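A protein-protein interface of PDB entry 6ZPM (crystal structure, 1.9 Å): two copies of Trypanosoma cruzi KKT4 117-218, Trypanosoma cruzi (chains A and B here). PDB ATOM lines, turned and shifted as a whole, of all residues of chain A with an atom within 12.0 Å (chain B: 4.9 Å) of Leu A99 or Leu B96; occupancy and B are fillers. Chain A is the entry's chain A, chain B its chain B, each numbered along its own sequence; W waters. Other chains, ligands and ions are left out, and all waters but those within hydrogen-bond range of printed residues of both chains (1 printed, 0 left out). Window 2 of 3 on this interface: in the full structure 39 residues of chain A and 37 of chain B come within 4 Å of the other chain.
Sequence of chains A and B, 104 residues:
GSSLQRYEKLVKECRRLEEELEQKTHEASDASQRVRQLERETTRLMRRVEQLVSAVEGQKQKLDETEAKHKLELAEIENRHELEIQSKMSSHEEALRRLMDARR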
ATOM      1  N   LYS A  88       2.493  39.512  -0.020  1.00  0.00           N
ATOM      2  CA  LYS A  88       3.215  38.328   0.437  1.00  0.00           C
ATOM      3  C   LYS A  88       2.718  37.078  -0.276  1.00  0.00           C
ATOM      4  O   LYS A  88       3.512  36.282  -0.788  1.00  0.00           O
ATOM      5  CB  LYS A  88       3.068  38.173   1.950  1.00  0.00           C
ATOM      6  CG  LYS A  88       4.015  39.039   2.761  1.00  0.00           C
ATOM      7  CD  LYS A  88       5.455  38.842   2.329  1.00  0.00           C
ATOM      8  CE  LYS A  88       6.418  39.307   3.413  1.00  0.00           C
ATOM      9  NZ  LYS A  88       6.019  40.629   3.970  1.00  0.00           N
ATOM     10  N   MET A  89       1.401  36.890  -0.328  1.00  0.00           N
ATOM     11  CA  MET A  89       0.890  35.680  -0.954  1.00  0.00           C
ATOM     12  C   MET A  89       1.203  35.650  -2.446  1.00  0.00           C
ATOM     13  O   MET A  89       1.516  34.583  -2.986  1.00  0.00           O
ATOM     14  CB  MET A  89      -0.604  35.549  -0.668  1.00  0.00           C
ATOM     15  CG  MET A  89      -0.881  35.526   0.838  1.00  0.00           C
ATOM     16  SD  MET A  89      -2.493  34.892   1.329  1.00  0.00           S
ATOM     17  CE  MET A  89      -2.293  33.152   0.937  1.00  0.00           C
ATOM     18  N   SER A  90       1.208  36.808  -3.107  1.00  0.00           N
ATOM     19  CA  SER A  90       1.543  36.848  -4.526  1.00  0.00           C
ATOM     20  C   SER A  90       3.025  36.571  -4.769  1.00  0.00           C
ATOM     21  O   SER A  90       3.385  35.932  -5.765  1.00  0.00           O
ATOM     22  CB  SER A  90       1.152  38.197  -5.120  1.00  0.00           C
ATOM     23  OG  SER A  90       1.959  38.497  -6.246  1.00  0.00           O
ATOM     24  N   SER A  91       3.904  37.061  -3.889  1.00  0.00           N
ATOM     25  CA  SER A  91       5.319  36.740  -4.038  1.00  0.00           C
ATOM     26  C   SER A  91       5.566  35.254  -3.813  1.00  0.00           C
ATOM     27  O   SER A  91       6.404  34.648  -4.492  1.00  0.00           O
ATOM     28  CB  SER A  91       6.169  37.584  -3.084  1.00  0.00           C
ATOM     29  OG  SER A  91       5.822  37.337  -1.736  1.00  0.00           O
ATOM     30  N   HIS A  92       4.834  34.648  -2.873  1.00  0.00           N
ATOM     31  CA  HIS A  92       4.982  33.217  -2.636  1.00  0.00           C
ATOM     32  C   HIS A  92       4.459  32.395  -3.811  1.00  0.00           C
ATOM     33  O   HIS A  92       5.002  31.325  -4.106  1.00  0.00           O
ATOM     34  CB  HIS A  92       4.274  32.830  -1.336  1.00  0.00           C
ATOM     35  CG  HIS A  92       4.885  33.436  -0.108  1.00  0.00           C
ATOM     36  ND1 HIS A  92       4.269  33.402   1.126  1.00  0.00           N
ATOM     37  CD2 HIS A  92       6.057  34.092   0.076  1.00  0.00           C
ATOM     38  CE1 HIS A  92       5.035  34.010   2.015  1.00  0.00           C
ATOM     39  NE2 HIS A  92       6.126  34.436   1.404  1.00  0.00           N
ATOM     40  N   GLU A  93       3.419  32.883  -4.500  1.00  0.00           N
ATOM     41  CA  GLU A  93       2.911  32.193  -5.684  1.00  0.00           C
ATOM     42  C   GLU A  93       3.885  32.288  -6.847  1.00  0.00           C
ATOM     43  O   GLU A  93       4.053  31.321  -7.604  1.00  0.00           O
ATOM     44  CB  GLU A  93       1.563  32.776  -6.107  1.00  0.00           C
ATOM     45  CG  GLU A  93       0.490  32.717  -5.046  1.00  0.00           C
ATOM     46  CD  GLU A  93      -0.298  31.427  -5.043  1.00  0.00           C
ATOM     47  OE1 GLU A  93       0.185  30.415  -5.597  1.00  0.00           O
ATOM     48  OE2 GLU A  93      -1.415  31.434  -4.487  1.00  0.00           O
ATOM     49  N   GLU A  94       4.501  33.457  -7.042  1.00  0.00           N
ATOM     50  CA  GLU A  94       5.541  33.566  -8.060  1.00  0.00           C
ATOM     51  C   GLU A  94       6.695  32.620  -7.756  1.00  0.00           C
ATOM     52  O   GLU A  94       7.171  31.900  -8.639  1.00  0.00           O
ATOM     53  CB  GLU A  94       6.035  35.009  -8.160  1.00  0.00           C
ATOM     54  CG  GLU A  94       5.550  35.739  -9.406  1.00  0.00           C
ATOM     55  CD  GLU A  94       5.939  35.028 -10.698  1.00  0.00           C
ATOM     56  OE1 GLU A  94       7.097  35.175 -11.144  1.00  0.00           O
ATOM     57  OE2 GLU A  94       5.087  34.312 -11.264  1.00  0.00           O
ATOM     58  N   ALA A  95       7.169  32.619  -6.504  1.00  0.00           N
ATOM     59  CA  ALA A  95       8.254  31.721  -6.115  1.00  0.00           C
ATOM     60  C   ALA A  95       7.896  30.270  -6.406  1.00  0.00           C
ATOM     61  O   ALA A  95       8.719  29.510  -6.929  1.00  0.00           O
ATOM     62  CB  ALA A  95       8.578  31.900  -4.630  1.00  0.00           C
ATOM     63  N   LEU A  96       6.663  29.875  -6.075  1.00  0.00           N
ATOM     64  CA  LEU A  96       6.178  28.534  -6.387  1.00  0.00           C
ATOM     65  C   LEU A  96       6.251  28.249  -7.880  1.00  0.00           C
ATOM     66  O   LEU A  96       6.731  27.190  -8.300  1.00  0.00           O
ATOM     67  CB  LEU A  96       4.737  28.383  -5.906  1.00  0.00           C
ATOM     68  CG  LEU A  96       4.469  27.654  -4.598  1.00  0.00           C
ATOM     69  CD1 LEU A  96       2.963  27.508  -4.418  1.00  0.00           C
ATOM     70  CD2 LEU A  96       5.148  26.304  -4.606  1.00  0.00           C
ATOM     71  N   ARG A  97       5.739  29.175  -8.696  1.00  0.00           N
ATOM     72  CA  ARG A  97       5.680  28.945 -10.136  1.00  0.00           C
ATOM     73  C   ARG A  97       7.076  28.800 -10.729  1.00  0.00           C
ATOM     74  O   ARG A  97       7.308  27.948 -11.597  1.00  0.00           O
ATOM     75  CB  ARG A  97       4.917  30.087 -10.807  1.00  0.00           C
ATOM     76  CG  ARG A  97       4.813  29.959 -12.313  1.00  0.00           C
ATOM     77  CD  ARG A  97       4.332  31.236 -12.981  1.00  0.00           C
ATOM     78  NE  ARG A  97       5.314  32.311 -12.895  1.00  0.00           N
ATOM     79  CZ  ARG A  97       6.365  32.440 -13.698  1.00  0.00           C
ATOM     80  NH1 ARG A  97       6.593  31.554 -14.657  1.00  0.00           N
ATOM     81  NH2 ARG A  97       7.194  33.461 -13.537  1.00  0.00           N
ATOM     82  N   ARG A  98       8.023  29.618 -10.269  1.00  0.00           N
ATOM     83  CA  ARG A  98       9.374  29.549 -10.814  1.00  0.00           C
ATOM     84  C   ARG A  98      10.089  28.282 -10.367  1.00  0.00           C
ATOM     85  O   ARG A  98      10.805  27.658 -11.160  1.00  0.00           O
ATOM     86  CB  ARG A  98      10.170  30.786 -10.399  1.00  0.00           C
ATOM     87  CG  ARG A  98       9.560  32.091 -10.894  1.00  0.00           C
ATOM     88  CD  ARG A  98      10.522  33.255 -10.703  1.00  0.00           C
ATOM     89  NE  ARG A  98       9.948  34.520 -11.152  1.00  0.00           N
ATOM     90  CZ  ARG A  98       9.892  34.909 -12.423  1.00  0.00           C
ATOM     91  NH1 ARG A  98      10.374  34.131 -13.380  1.00  0.00           N
ATOM     92  NH2 ARG A  98       9.351  36.079 -12.739  1.00  0.00           N
ATOM     93  N   LEU A  99       9.920  27.891  -9.101  1.00  0.00           N
ATOM     94  CA  LEU A  99      10.612  26.703  -8.610  1.00  0.00           C
ATOM     95  C   LEU A  99      10.047  25.437  -9.240  1.00  0.00           C
ATOM     96  O   LEU A  99      10.797  24.503  -9.550  1.00  0.00           O
ATOM     97  CB  LEU A  99      10.533  26.639  -7.084  1.00  0.00           C
ATOM     98  CG  LEU A  99      11.410  27.652  -6.344  1.00  0.00           C
ATOM     99  CD1 LEU A  99      11.147  27.611  -4.843  1.00  0.00           C
ATOM    100  CD2 LEU A  99      12.887  27.410  -6.645  1.00  0.00           C
ATOM    101  N   MET A 100       8.732  25.392  -9.465  1.00  0.00           N
ATOM    102  CA  MET A 100       8.177  24.250 -10.183  1.00  0.00           C
ATOM    103  C   MET A 100       8.656  24.222 -11.636  1.00  0.00           C
ATOM    104  O   MET A 100       8.869  23.139 -12.193  1.00  0.00           O
ATOM    105  CB  MET A 100       6.649  24.268 -10.090  1.00  0.00           C
ATOM    106  CG  MET A 100       6.116  24.065  -8.660  1.00  0.00           C
ATOM    107  SD  MET A 100       6.629  22.508  -7.883  1.00  0.00           S
ATOM    108  CE  MET A 100       7.916  23.048  -6.760  1.00  0.00           C
ATOM    109  N   ASP A 101       8.865  25.397 -12.248  1.00  0.00           N
ATOM    110  CA  ASP A 101       9.475  25.460 -13.579  1.00  0.00           C
ATOM    111  C   ASP A 101      10.903  24.933 -13.571  1.00  0.00           C
ATOM    112  O   ASP A 101      11.332  24.263 -14.520  1.00  0.00           O
ATOM    113  CB  ASP A 101       9.482  26.897 -14.092  1.00  0.00           C
ATOM    114  CG  ASP A 101       8.228  27.257 -14.852  1.00  0.00           C
ATOM    115  OD1 ASP A 101       7.392  26.363 -15.080  1.00  0.00           O
ATOM    116  OD2 ASP A 101       8.074  28.444 -15.202  1.00  0.00           O
ATOM    117  N   ALA A 102      11.665  25.262 -12.528  1.00  0.00           N
ATOM    118  CA  ALA A 102      13.070  24.874 -12.482  1.00  0.00           C
ATOM    119  C   ALA A 102      13.228  23.366 -12.375  1.00  0.00           C
ATOM    120  O   ALA A 102      14.109  22.780 -13.019  1.00  0.00           O
ATOM    121  CB  ALA A 102      13.764  25.570 -11.310  1.00  0.00           C
ATOM    122  N   ARG A 103      12.387  22.716 -11.578  1.00  0.00           N
ATOM    123  CA  ARG A 103      12.522  21.280 -11.380  1.00  0.00           C
ATOM    124  C   ARG A 103      11.884  20.468 -12.500  1.00  0.00           C
ATOM    125  O   ARG A 103      11.892  19.234 -12.427  1.00  0.00           O
ATOM    126  CB  ARG A 103      11.928  20.880 -10.024  1.00  0.00           C
ATOM    127  CG  ARG A 103      10.453  21.185  -9.870  1.00  0.00           C
ATOM    128  CD  ARG A 103       9.884  20.558  -8.603  1.00  0.00           C
ATOM    129  NE  ARG A 103       9.990  19.097  -8.596  1.00  0.00           N
ATOM    130  CZ  ARG A 103       9.190  18.280  -9.278  1.00  0.00           C
ATOM    131  NH1 ARG A 103       8.220  18.771 -10.035  1.00  0.00           N
ATOM    132  NH2 ARG A 103       9.361  16.967  -9.204  1.00  0.00           N
ATOM    133  N   ARG A 104      11.367  21.124 -13.538  1.00  0.00           N
ATOM    134  CA  ARG A 104      10.633  20.461 -14.614  1.00  0.00           C
ATOM    135  C   ARG A 104      11.512  19.493 -15.408  1.00  0.00           C
ATOM    136  O   ARG A 104      12.569  19.874 -15.915  1.00  0.00           O
ATOM    137  CB  ARG A 104      10.023  21.505 -15.555  1.00  0.00           C
ATOM    138  CG  ARG A 104       8.558  21.266 -15.880  1.00  0.00           C
ATOM    139  CD  ARG A 104       7.888  22.480 -16.536  1.00  0.00           C
ATOM    140  NE  ARG A 104       7.177  23.325 -15.578  1.00  0.00           N
ATOM    141  CZ  ARG A 104       6.059  22.964 -14.956  1.00  0.00           C
ATOM    142  NH1 ARG A 104       5.530  21.772 -15.190  1.00  0.00           N
ATOM    143  NH2 ARG A 104       5.472  23.790 -14.100  1.00  0.00           N
ATOM    144  N   HIS B  92       5.323  29.332   4.230  1.00  0.00           N
ATOM    145  CA  HIS B  92       5.918  29.329   2.897  1.00  0.00           C
ATOM    146  C   HIS B  92       7.251  28.591   2.892  1.00  0.00           C
ATOM    147  O   HIS B  92       7.542  27.827   1.966  1.00  0.00           O
ATOM    148  CB  HIS B  92       6.075  30.772   2.408  1.00  0.00           C
ATOM    149  CG  HIS B  92       7.191  30.979   1.427  1.00  0.00           C
ATOM    150  ND1 HIS B  92       6.993  30.981   0.063  1.00  0.00           N
ATOM    151  CD2 HIS B  92       8.509  31.227   1.614  1.00  0.00           C
ATOM    152  CE1 HIS B  92       8.142  31.207  -0.549  1.00  0.00           C
ATOM    153  NE2 HIS B  92       9.079  31.355   0.369  1.00  0.00           N
ATOM    154  N   GLU B  93       8.066  28.793   3.931  1.00  0.00           N
ATOM    155  CA  GLU B  93       9.353  28.110   4.019  1.00  0.00           C
ATOM    156  C   GLU B  93       9.178  26.603   4.161  1.00  0.00           C
ATOM    157  O   GLU B  93       9.904  25.827   3.528  1.00  0.00           O
ATOM    158  CB  GLU B  93      10.153  28.668   5.195  1.00  0.00           C
ATOM    159  CG  GLU B  93      11.630  28.319   5.187  1.00  0.00           C
ATOM    160  CD  GLU B  93      12.346  28.859   6.407  1.00  0.00           C
ATOM    161  OE1 GLU B  93      13.374  28.270   6.808  1.00  0.00           O
ATOM    162  OE2 GLU B  93      11.871  29.869   6.969  1.00  0.00           O
ATOM    163  N   GLU B  94       8.233  26.166   4.993  1.00  0.00           N
ATOM    164  CA  GLU B  94       7.963  24.737   5.105  1.00  0.00           C
ATOM    165  C   GLU B  94       7.447  24.176   3.784  1.00  0.00           C
ATOM    166  O   GLU B  94       7.839  23.075   3.374  1.00  0.00           O
ATOM    167  CB  GLU B  94       6.973  24.475   6.243  1.00  0.00           C
ATOM    168  CG  GLU B  94       6.065  23.261   6.051  1.00  0.00           C
ATOM    169  CD  GLU B  94       6.701  21.957   6.513  1.00  0.00           C
ATOM    170  OE1 GLU B  94       7.880  21.977   6.936  1.00  0.00           O
ATOM    171  OE2 GLU B  94       6.013  20.911   6.460  1.00  0.00           O
ATOM    172  N   ALA B  95       6.587  24.926   3.090  1.00  0.00           N
ATOM    173  CA  ALA B  95       6.096  24.474   1.790  1.00  0.00           C
ATOM    174  C   ALA B  95       7.244  24.284   0.808  1.00  0.00           C
ATOM    175  O   ALA B  95       7.340  23.248   0.139  1.00  0.00           O
ATOM    176  CB  ALA B  95       5.073  25.466   1.238  1.00  0.00           C
ATOM    177  N   LEU B  96       8.132  25.278   0.711  1.00  0.00           N
ATOM    178  CA  LEU B  96       9.264  25.175  -0.206  1.00  0.00           C
ATOM    179  C   LEU B  96      10.179  24.020   0.173  1.00  0.00           C
ATOM    180  O   LEU B  96      10.711  23.327  -0.702  1.00  0.00           O
ATOM    181  CB  LEU B  96      10.049  26.487  -0.225  1.00  0.00           C
ATOM    182  CG  LEU B  96       9.787  27.452  -1.383  1.00  0.00           C
ATOM    183  CD1 LEU B  96       8.293  27.635  -1.633  1.00  0.00           C
ATOM    184  CD2 LEU B  96      10.468  28.789  -1.128  1.00  0.00           C
ATOM    185  N   ARG B  97      10.375  23.799   1.473  1.00  0.00           N
ATOM    186  CA  ARG B  97      11.229  22.710   1.930  1.00  0.00           C
ATOM    187  C   ARG B  97      10.635  21.350   1.583  1.00  0.00           C
ATOM    188  O   ARG B  97      11.367  20.408   1.264  1.00  0.00           O
ATOM    189  CB  ARG B  97      11.455  22.832   3.436  1.00  0.00           C
ATOM    190  CG  ARG B  97      12.377  21.784   4.020  1.00  0.00           C
ATOM    191  CD  ARG B  97      12.327  21.784   5.540  1.00  0.00           C
ATOM    192  NE  ARG B  97      12.274  23.130   6.102  1.00  0.00           N
ATOM    193  CZ  ARG B  97      11.245  23.614   6.794  1.00  0.00           C
ATOM    194  NH1 ARG B  97      10.177  22.858   7.012  1.00  0.00           N
ATOM    195  NH2 ARG B  97      11.284  24.854   7.272  1.00  0.00           N
ATOM    196  N   ARG B  98       9.311  21.222   1.642  1.00  0.00           N
ATOM    197  CA  ARG B  98       8.694  19.946   1.310  1.00  0.00           C
ATOM    198  C   ARG B  98       8.600  19.726  -0.195  1.00  0.00           C
ATOM    199  O   ARG B  98       8.618  18.576  -0.648  1.00  0.00           O
ATOM    200  CB  ARG B  98       7.311  19.853   1.943  1.00  0.00           C
ATOM    201  CG  ARG B  98       7.359  19.572   3.429  1.00  0.00           C
ATOM    202  CD  ARG B  98       6.393  18.482   3.793  1.00  0.00           C
ATOM    203  NE  ARG B  98       6.488  18.085   5.195  1.00  0.00           N
ATOM    204  CZ  ARG B  98       6.999  16.934   5.621  1.00  0.00           C
ATOM    205  NH1 ARG B  98       7.468  16.048   4.752  1.00  0.00           N
ATOM    206  NH2 ARG B  98       7.025  16.662   6.919  1.00  0.00           N
ATOM    207  N   LEU B  99       8.505  20.800  -0.980  1.00  0.00           N
ATOM    208  CA  LEU B  99       8.409  20.642  -2.427  1.00  0.00           C
ATOM    209  C   LEU B  99       9.774  20.465  -3.079  1.00  0.00           C
ATOM    210  O   LEU B  99       9.887  19.764  -4.087  1.00  0.00           O
ATOM    211  CB  LEU B  99       7.678  21.841  -3.037  1.00  0.00           C
ATOM    212  CG  LEU B  99       6.166  21.834  -2.797  1.00  0.00           C
ATOM    213  CD1 LEU B  99       5.597  23.246  -2.776  1.00  0.00           C
ATOM    214  CD2 LEU B  99       5.459  20.977  -3.843  1.00  0.00           C
ATOM    215  N   MET B 100      10.807  21.070  -2.513  1.00  0.00           N
ATOM    216  CA  MET B 100      12.159  21.057  -3.112  1.00  0.00           C
ATOM    217  C   MET B 100      13.032  20.022  -2.425  1.00  0.00           C
ATOM    218  O   MET B 100      14.025  19.623  -2.980  1.00  0.00           O
ATOM    219  CB  MET B 100      12.824  22.430  -2.990  1.00  0.00           C
ATOM    220  CG  MET B 100      12.021  23.496  -3.664  1.00  0.00           C
ATOM    221  SD  MET B 100      11.617  23.058  -5.347  1.00  0.00           S
ATOM    222  CE  MET B 100      13.258  22.801  -5.996  1.00  0.00           C
ATOM    223  N   ASP B 101      12.619  19.666  -1.228  1.00  0.00           N
ATOM    224  CA  ASP B 101      13.244  18.632  -0.387  1.00  0.00           C
ATOM    225  C   ASP B 101      14.633  19.115   0.032  1.00  0.00           C
ATOM    226  O   ASP B 101      14.717  19.661   1.126  1.00  0.00           O
ATOM    227  CB  ASP B 101      13.065  17.264  -1.042  1.00  0.00           C
ATOM    228  CG  ASP B 101      13.200  16.167  -0.043  1.00  0.00           C
ATOM    229  OD1 ASP B 101      13.218  16.506   1.143  1.00  0.00           O
ATOM    230  OD2 ASP B 101      13.307  15.001  -0.479  1.00  0.00           O
HETATM  231  O   HOH W   1      11.268  18.273  -6.250  1.00  0.00           O
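Of the 10 printed residues of chain B, 4 touch a printed residue of chain A. Of the 17 printed residues of chain A, 4 touch a printed residue of chain B. Printed residues of chain A that touch a printed residue of chain B: His A92, Leu A96, Leu A99 and Met A100. Hydrophobic or aromatic side chains of chain A within 4 Å of the printed part of chain B: His A92, Leu A96, Leu A99 and Met A100.
His A92 touches its own counterpart, His B92. Leu A96 touches Leu B99, and with the chains exchanged Leu A99 touches Leu B96. Met A100 touches Leu B99, but with the chains exchanged Leu A99 does not touch Met B100 (4.1 Å). Met A100 touches its own counterpart, Met B100. 10 positions are printed for both chains. Of the 5 pairs that touch across the chains among the printed residues, 4 have their exchanged pair printed and touching as well.
Water W1 bridges NE of Arg A103 (2.8 Å) and O of Leu B99 (3.0 Å).
Leu A99 touches just one residue of chain B: Leu B96. Of the printed residues of chain A, Leu B96 touches Leu A99 (3.7 Å). No residue of chain A comes within 4 Å of Glu B94. No residue of chain A comes within 4 Å of Arg B97. Of chain A, only Met A100 (3.96 Å) comes within 4 Å of Met B100. Of the printed residues of chain B, Leu A96 touches Leu B99. Of the printed residues of chain B, His A92 touches His B92 (3.2 Å). Of the printed residues of chain B, Met A100 touches Leu B99 and Met B100. Of the printed residues of chain A, His B92 touches His A92. Asp B101 touches none of the printed residues of chain A. Arg A103 touches none of the printed residues of chain B. The nearest residue of chain A that does not touch Leu B96 is Leu A96 (4.5 Å).
Among the printed residues, pairs that only touch across the chains: His A92 with His B92 (3.2 Å), Leu A96 with Leu B99 (3.6 Å), Leu A99 with Leu B96 (3.7 Å), Met A100 with Leu B99 (3.9 Å) and Met A100 with Met B100 (3.96 Å).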
